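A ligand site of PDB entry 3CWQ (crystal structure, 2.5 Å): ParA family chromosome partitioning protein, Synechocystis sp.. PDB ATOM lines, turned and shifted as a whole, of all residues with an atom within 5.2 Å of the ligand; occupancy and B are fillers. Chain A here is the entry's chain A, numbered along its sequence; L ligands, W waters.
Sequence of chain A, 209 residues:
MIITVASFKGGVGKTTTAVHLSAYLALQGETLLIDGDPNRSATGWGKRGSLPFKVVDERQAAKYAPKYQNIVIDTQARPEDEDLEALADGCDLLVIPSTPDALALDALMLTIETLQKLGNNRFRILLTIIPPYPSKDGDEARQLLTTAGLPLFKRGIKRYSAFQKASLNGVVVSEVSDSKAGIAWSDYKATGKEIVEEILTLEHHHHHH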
ATOM      1  N   SER A   7      24.660  21.968  24.451  1.00  0.00           N
ATOM      2  CA  SER A   7      23.345  22.532  24.507  1.00  0.00           C
ATOM      3  C   SER A   7      22.779  22.588  25.927  1.00  0.00           C
ATOM      4  O   SER A   7      23.269  21.950  26.860  1.00  0.00           O
ATOM      5  CB  SER A   7      22.426  21.703  23.613  1.00  0.00           C
ATOM      6  OG  SER A   7      22.366  20.423  24.136  1.00  0.00           O
ATOM      7  N   LYS A   9      19.444  21.820  26.276  1.00  0.00           N
ATOM      8  CA  LYS A   9      18.219  21.049  26.204  1.00  0.00           C
ATOM      9  C   LYS A   9      18.321  19.971  25.113  1.00  0.00           C
ATOM     10  O   LYS A   9      19.111  20.047  24.152  1.00  0.00           O
ATOM     11  CB  LYS A   9      16.978  21.977  26.008  1.00  0.00           C
ATOM     12  CG  LYS A   9      15.929  21.795  27.097  1.00  0.00           C
ATOM     13  CD  LYS A   9      14.525  22.307  26.790  1.00  0.00           C
ATOM     14  CE  LYS A   9      14.229  22.363  25.268  1.00  0.00           C
ATOM     15  NZ  LYS A   9      13.383  21.328  24.567  1.00  0.00           N
ATOM     16  N   GLY A  10      17.555  18.915  25.262  1.00  0.00           N
ATOM     17  CA  GLY A  10      17.543  17.901  24.223  1.00  0.00           C
ATOM     18  C   GLY A  10      16.631  18.444  23.168  1.00  0.00           C
ATOM     19  O   GLY A  10      15.770  19.240  23.476  1.00  0.00           O
ATOM     20  N   GLY A  11      16.812  18.016  21.929  1.00  0.00           N
ATOM     21  CA  GLY A  11      15.863  18.304  20.870  1.00  0.00           C
ATOM     22  C   GLY A  11      16.079  19.634  20.180  1.00  0.00           C
ATOM     23  O   GLY A  11      15.141  20.167  19.522  1.00  0.00           O
ATOM     24  N   VAL A  12      17.325  20.129  20.280  1.00  0.00           N
ATOM     25  CA  VAL A  12      17.708  21.358  19.633  1.00  0.00           C
ATOM     26  C   VAL A  12      18.626  21.156  18.456  1.00  0.00           C
ATOM     27  O   VAL A  12      19.097  22.137  17.932  1.00  0.00           O
ATOM     28  CB  VAL A  12      18.407  22.372  20.626  1.00  0.00           C
ATOM     29  CG1 VAL A  12      17.504  22.741  21.716  1.00  0.00           C
ATOM     30  CG2 VAL A  12      19.649  21.837  21.147  1.00  0.00           C
ATOM     31  N   GLY A  13      18.935  19.939  18.032  1.00  0.00           N
ATOM     32  CA  GLY A  13      19.789  19.721  16.820  1.00  0.00           C
ATOM     33  C   GLY A  13      21.295  19.766  17.122  1.00  0.00           C
ATOM     34  O   GLY A  13      22.121  19.768  16.191  1.00  0.00           O
ATOM     35  N   LYS A  14      21.663  19.758  18.400  1.00  0.00           N
ATOM     36  CA  LYS A  14      23.042  19.607  18.796  1.00  0.00           C
ATOM     37  C   LYS A  14      23.743  18.450  18.091  1.00  0.00           C
ATOM     38  O   LYS A  14      24.595  18.642  17.242  1.00  0.00           O
ATOM     39  CB  LYS A  14      23.127  19.472  20.326  1.00  0.00           C
ATOM     40  CG  LYS A  14      24.547  19.149  20.916  1.00  0.00           C
ATOM     41  CD  LYS A  14      24.439  18.754  22.456  1.00  0.00           C
ATOM     42  CE  LYS A  14      23.497  17.465  22.734  1.00  0.00           C
ATOM     43  NZ  LYS A  14      23.825  16.364  21.832  1.00  0.00           N
ATOM     44  N   THR A  15      23.426  17.244  18.439  1.00  0.00           N
ATOM     45  CA  THR A  15      23.978  16.127  17.681  1.00  0.00           C
ATOM     46  C   THR A  15      24.050  16.362  16.160  1.00  0.00           C
ATOM     47  O   THR A  15      25.094  16.174  15.593  1.00  0.00           O
ATOM     48  CB  THR A  15      23.285  14.805  18.028  1.00  0.00           C
ATOM     49  OG1 THR A  15      23.749  14.356  19.319  1.00  0.00           O
ATOM     50  CG2 THR A  15      23.829  13.736  17.156  1.00  0.00           C
ATOM     51  N   THR A  16      22.961  16.802  15.535  1.00  0.00           N
ATOM     52  CA  THR A  16      22.844  17.088  14.096  1.00  0.00           C
ATOM     53  C   THR A  16      23.859  18.173  13.647  1.00  0.00           C
ATOM     54  O   THR A  16      24.463  18.115  12.539  1.00  0.00           O
ATOM     55  CB  THR A  16      21.415  17.635  13.841  1.00  0.00           C
ATOM     56  OG1 THR A  16      20.409  16.638  14.143  1.00  0.00           O
ATOM     57  CG2 THR A  16      21.171  18.026  12.335  1.00  0.00           C
ATOM     58  N   ASP A  37      26.964  12.200  24.343  1.00  0.00           N
ATOM     59  CA  ASP A  37      25.541  12.362  24.562  1.00  0.00           C
ATOM     60  C   ASP A  37      24.997  11.057  25.093  1.00  0.00           C
ATOM     61  O   ASP A  37      25.014  10.027  24.356  1.00  0.00           O
ATOM     62  CB  ASP A  37      24.816  12.701  23.271  1.00  0.00           C
ATOM     63  CG  ASP A  37      23.342  13.046  23.518  1.00  0.00           C
ATOM     64  OD1 ASP A  37      22.738  13.731  22.662  1.00  0.00           O
ATOM     65  OD2 ASP A  37      22.665  12.724  24.538  1.00  0.00           O
ATOM     66  N   ASN A  39      22.362   9.619  24.845  1.00  0.00           N
ATOM     67  CA  ASN A  39      21.572   8.800  23.917  1.00  0.00           C
ATOM     68  C   ASN A  39      22.483   8.153  22.852  1.00  0.00           C
ATOM     69  O   ASN A  39      21.999   7.242  22.134  1.00  0.00           O
ATOM     70  CB  ASN A  39      20.402   9.554  23.246  1.00  0.00           C
ATOM     71  CG  ASN A  39      20.853  10.817  22.396  1.00  0.00           C
ATOM     72  OD1 ASN A  39      22.040  10.928  21.890  1.00  0.00           O
ATOM     73  ND2 ASN A  39      19.896  11.777  22.228  1.00  0.00           N
ATOM     74  N   SER A  41      23.271   9.030  20.112  1.00  0.00           N
ATOM     75  CA  SER A  41      22.564   9.117  18.841  1.00  0.00           C
ATOM     76  C   SER A  41      23.594   9.271  17.731  1.00  0.00           C
ATOM     77  O   SER A  41      23.357   8.846  16.557  1.00  0.00           O
ATOM     78  CB  SER A  41      21.525  10.254  18.886  1.00  0.00           C
ATOM     79  OG  SER A  41      21.971  11.514  18.387  1.00  0.00           O
ATOM     80  N   ASP A  74      30.394  16.160  20.867  1.00  0.00           N
ATOM     81  CA  ASP A  74      28.918  16.365  20.981  1.00  0.00           C
ATOM     82  C   ASP A  74      28.511  16.032  22.401  1.00  0.00           C
ATOM     83  O   ASP A  74      28.522  14.851  22.783  1.00  0.00           O
ATOM     84  CB  ASP A  74      28.236  15.445  19.960  1.00  0.00           C
ATOM     85  CG  ASP A  74      26.735  15.198  20.209  1.00  0.00           C
ATOM     86  OD1 ASP A  74      26.218  14.302  19.540  1.00  0.00           O
ATOM     87  OD2 ASP A  74      25.970  15.836  20.984  1.00  0.00           O
ATOM     88  N   ILE A 129      16.877  24.779  13.511  1.00  0.00           N
ATOM     89  CA  ILE A 129      15.513  24.340  13.231  1.00  0.00           C
ATOM     90  C   ILE A 129      14.559  25.529  13.263  1.00  0.00           C
ATOM     91  O   ILE A 129      13.463  25.430  13.788  1.00  0.00           O
ATOM     92  CB  ILE A 129      15.042  23.241  14.257  1.00  0.00           C
ATOM     93  CG1 ILE A 129      16.193  22.450  14.787  1.00  0.00           C
ATOM     94  CG2 ILE A 129      14.050  22.263  13.591  1.00  0.00           C
ATOM     95  CD1 ILE A 129      15.759  21.585  15.940  1.00  0.00           C
ATOM     96  N   ILE A 157      20.167  27.479  11.191  1.00  0.00           N
ATOM     97  CA  ILE A 157      19.734  26.321  10.420  1.00  0.00           C
ATOM     98  C   ILE A 157      18.231  26.286  10.215  1.00  0.00           C
ATOM     99  O   ILE A 157      17.488  26.424  11.187  1.00  0.00           O
ATOM    100  CB  ILE A 157      20.158  25.038  11.102  1.00  0.00           C
ATOM    101  CG1 ILE A 157      21.624  25.124  11.537  1.00  0.00           C
ATOM    102  CG2 ILE A 157      19.969  23.947  10.136  1.00  0.00           C
ATOM    103  CD1 ILE A 157      22.656  25.601  10.409  1.00  0.00           C
ATOM    104  N   LYS A 158      17.734  26.129   8.990  1.00  0.00           N
ATOM    105  CA  LYS A 158      16.264  26.090   8.817  1.00  0.00           C
ATOM    106  C   LYS A 158      15.695  24.712   9.129  1.00  0.00           C
ATOM    107  O   LYS A 158      16.417  23.731   9.100  1.00  0.00           O
ATOM    108  CB  LYS A 158      15.802  26.589   7.438  1.00  0.00           C
ATOM    109  CG  LYS A 158      16.264  28.020   6.981  1.00  0.00           C
ATOM    110  CD  LYS A 158      16.188  29.183   8.048  1.00  0.00           C
ATOM    111  CE  LYS A 158      15.793  30.574   7.386  1.00  0.00           C
ATOM    112  NZ  LYS A 158      14.420  30.560   6.675  1.00  0.00           N
ATOM    113  N   ARG A 159      14.412  24.604   9.452  1.00  0.00           N
ATOM    114  CA  ARG A 159      13.854  23.262   9.590  1.00  0.00           C
ATOM    115  C   ARG A 159      13.662  22.723   8.189  1.00  0.00           C
ATOM    116  O   ARG A 159      12.925  23.305   7.399  1.00  0.00           O
ATOM    117  CB  ARG A 159      12.548  23.276  10.359  1.00  0.00           C
ATOM    118  CG  ARG A 159      11.852  21.881  10.523  1.00  0.00           C
ATOM    119  CD  ARG A 159      10.525  21.900  11.323  1.00  0.00           C
ATOM    120  NE  ARG A 159       9.645  23.016  10.931  1.00  0.00           N
ATOM    121  CZ  ARG A 159       8.645  22.960  10.001  1.00  0.00           C
ATOM    122  NH1 ARG A 159       7.890  24.052   9.738  1.00  0.00           N
ATOM    123  NH2 ARG A 159       8.394  21.811   9.320  1.00  0.00           N
ATOM    124  N   TYR A 160      14.385  21.659   7.833  1.00  0.00           N
ATOM    125  CA  TYR A 160      14.151  20.987   6.534  1.00  0.00           C
ATOM    126  C   TYR A 160      13.928  19.596   6.913  1.00  0.00           C
ATOM    127  O   TYR A 160      14.683  19.054   7.709  1.00  0.00           O
ATOM    128  CB  TYR A 160      15.344  21.031   5.598  1.00  0.00           C
ATOM    129  CG  TYR A 160      15.612  22.429   5.110  1.00  0.00           C
ATOM    130  CD1 TYR A 160      16.759  23.125   5.505  1.00  0.00           C
ATOM    131  CD2 TYR A 160      14.638  23.094   4.289  1.00  0.00           C
ATOM    132  CE1 TYR A 160      16.952  24.462   5.072  1.00  0.00           C
ATOM    133  CE2 TYR A 160      14.840  24.415   3.831  1.00  0.00           C
ATOM    134  CZ  TYR A 160      16.000  25.085   4.231  1.00  0.00           C
ATOM    135  OH  TYR A 160      16.174  26.369   3.771  1.00  0.00           O
ATOM    136  N   SER A 161      12.867  19.039   6.370  1.00  0.00           N
ATOM    137  CA  SER A 161      12.541  17.672   6.620  1.00  0.00           C
ATOM    138  C   SER A 161      13.772  16.806   6.285  1.00  0.00           C
ATOM    139  O   SER A 161      14.047  15.831   6.991  1.00  0.00           O
ATOM    140  CB  SER A 161      11.288  17.292   5.802  1.00  0.00           C
ATOM    141  OG  SER A 161      10.597  16.227   6.445  1.00  0.00           O
ATOM    142  N   PHE A 163      16.929  16.985   7.040  1.00  0.00           N
ATOM    143  CA  PHE A 163      17.786  16.672   8.159  1.00  0.00           C
ATOM    144  C   PHE A 163      17.430  15.366   8.809  1.00  0.00           C
ATOM    145  O   PHE A 163      18.263  14.641   9.324  1.00  0.00           O
ATOM    146  CB  PHE A 163      17.867  17.846   9.204  1.00  0.00           C
ATOM    147  CG  PHE A 163      18.811  18.930   8.782  1.00  0.00           C
ATOM    148  CD1 PHE A 163      20.136  18.631   8.474  1.00  0.00           C
ATOM    149  CD2 PHE A 163      18.369  20.222   8.599  1.00  0.00           C
ATOM    150  CE1 PHE A 163      21.015  19.604   7.994  1.00  0.00           C
ATOM    151  CE2 PHE A 163      19.268  21.234   8.161  1.00  0.00           C
ATOM    152  CZ  PHE A 163      20.584  20.915   7.851  1.00  0.00           C
ATOM    153  N   GLN A 164      16.155  15.054   8.736  1.00  0.00           N
ATOM    154  CA  GLN A 164      15.636  13.850   9.318  1.00  0.00           C
ATOM    155  C   GLN A 164      16.017  12.605   8.544  1.00  0.00           C
ATOM    156  O   GLN A 164      16.381  11.578   9.145  1.00  0.00           O
ATOM    157  CB  GLN A 164      14.120  13.951   9.342  1.00  0.00           C
ATOM    158  CG  GLN A 164      13.573  13.495  10.634  1.00  0.00           C
ATOM    159  CD  GLN A 164      12.634  14.521  11.234  1.00  0.00           C
ATOM    160  OE1 GLN A 164      13.045  15.652  11.644  1.00  0.00           O
ATOM    161  NE2 GLN A 164      11.360  14.128  11.326  1.00  0.00           N
ATOM    162  N   SER A 167      19.357  11.624   9.138  1.00  0.00           N
ATOM    163  CA  SER A 167      19.372  10.768  10.333  1.00  0.00           C
ATOM    164  C   SER A 167      19.013   9.242  10.048  1.00  0.00           C
ATOM    165  O   SER A 167      19.833   8.312  10.243  1.00  0.00           O
ATOM    166  CB  SER A 167      18.438  11.416  11.361  1.00  0.00           C
ATOM    167  OG  SER A 167      18.966  11.222  12.632  1.00  0.00           O
HETATM  168  P1  LIG L   1      19.925  17.264  20.137  1.00  0.00           P
HETATM  169  O1  LIG L   1      21.324  17.222  19.608  1.00  0.00           O
HETATM  170  O2  LIG L   1      19.896  18.349  21.269  1.00  0.00           O
HETATM  171  O3  LIG L   1      19.661  15.869  20.502  1.00  0.00           O
HETATM  172  P2  LIG L   1      18.911  16.182  17.618  1.00  0.00           P
HETATM  173  O4  LIG L   1      19.777  16.693  16.496  1.00  0.00           O
HETATM  174  O5  LIG L   1      19.067  14.717  17.967  1.00  0.00           O
HETATM  175  O6  LIG L   1      18.902  17.214  18.935  1.00  0.00           O
HETATM  176  O7  LIG L   1      17.439  16.586  17.079  1.00  0.00           O
HETATM  177  C1  LIG L   1      16.513  15.517  17.009  1.00  0.00           C
HETATM  178  C2  LIG L   1      15.605  15.551  15.779  1.00  0.00           C
HETATM  179  O8  LIG L   1      15.381  16.881  15.292  1.00  0.00           O
HETATM  180  C3  LIG L   1      16.304  14.777  14.675  1.00  0.00           C
HETATM  181  O9  LIG L   1      15.487  13.660  14.288  1.00  0.00           O
HETATM  182  C4  LIG L   1      16.365  15.677  13.485  1.00  0.00           C
HETATM  183  O10 LIG L   1      15.501  15.092  12.461  1.00  0.00           O
HETATM  184  C5  LIG L   1      15.590  16.917  13.878  1.00  0.00           C
HETATM  185  N1  LIG L   1      16.331  18.069  13.375  1.00  0.00           N
HETATM  186  C6  LIG L   1      17.461  18.592  13.865  1.00  0.00           C
HETATM  187  N2  LIG L   1      17.768  19.678  13.137  1.00  0.00           N
HETATM  188  C7  LIG L   1      16.858  19.867  12.176  1.00  0.00           C
HETATM  189  C8  LIG L   1      16.650  20.796  11.093  1.00  0.00           C
HETATM  190  N3  LIG L   1      17.506  21.794  10.846  1.00  0.00           N
HETATM  191  N4  LIG L   1      15.578  20.617  10.297  1.00  0.00           N
HETATM  192  C9  LIG L   1      14.746  19.621  10.482  1.00  0.00           C
HETATM  193  N5  LIG L   1      14.883  18.741  11.467  1.00  0.00           N
HETATM  194  C10 LIG L   1      15.926  18.798  12.321  1.00  0.00           C
HETATM  195  O   HOH W   1      20.200  12.800  16.454  1.00  0.00           O
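The side-chain amino group of Lys 14 lies within salt-bridge range of the side-chain carboxylate of Asp 37, at 3.0 Å.
The side-chain amino group of Lys 14 sits at hydrogen-bond distance from the side-chain hydroxyl of Thr 15, at 3.2 Å.
The side-chain amino group (NZ) of Lys 14 is in salt-bridge range of the side-chain carboxylate (OD1) of Asp 74 (3.9 Å).
The backbone carbonyl oxygen (O) of Lys 9 sits at hydrogen-bond distance from the side-chain hydroxyl (OG) of Ser 7 (3.3 Å).
The side-chain hydroxyl of Thr 15 sits close to the side-chain hydroxyl of Ser 41, at 3.5 Å.
The backbone carbonyl oxygen of Ile 157 lies within hydrogen-bond range of the backbone NH of Ile 129.
The side-chain carboxylate (OD1) of Asp 74 is in hydrogen-bond range of the side-chain hydroxyl (OG1) of Thr 15 (2.5 Å).
Water W1 lies within hydrogen-bond range of O5 of the ligand (2.7 Å) and OG of Ser 41 (2.9 Å).
O1 of the ligand lies within salt-bridge range of NZ of Lys 14 (3.5 Å).
An oxygen (O1) of the ligand is in hydrogen-bond range of the backbone NH (N) of Lys 14.
An oxygen (O4) of the ligand lies close to the backbone NH of Thr 16, 3.3 Å away.
The backbone NH (N) of Gly 11 lies within hydrogen-bond range of an oxygen (O2) of the ligand, 3.2 Å away.
An oxygen (O4) of the ligand lies within hydrogen-bond range of the side-chain hydroxyl (OG1) of Thr 16.
The backbone NH (N) of Thr 15 is in hydrogen-bond range of an oxygen (O1) of the ligand, at 2.4 Å.
N3 of the ligand sits at hydrogen-bond distance from O of Lys 158 (2.8 Å).
N of Tyr 160 sits at hydrogen-bond distance from N4 of the ligand (2.9 Å).
O10 of the ligand is in hydrogen-bond range of OE1 of Gln 164.
An oxygen (O6) of the ligand is in hydrogen-bond range of the backbone NH of Gly 13.
The backbone NH (N) of Val 12 lies within hydrogen-bond range of an oxygen (O2) of the ligand (3.3 Å).
An oxygen (O2) of the ligand sits close to the backbone carbonyl oxygen (O) of Lys 9 (3.4 Å).
Merely in contact with the ligand: Phe 163 (2.9 Å), Arg 159 (3.2 Å), Ile 157 (3.3 Å), Ile 129 (3.6 Å) and Gly 10 (3.8 Å).
Hydrophobic or aromatic side chains within 4 Å of the ligand: Val 12, Ile 129, Ile 157 and Phe 163.
Of the 22 residues printed, 15 come within 4 Å of the ligand.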
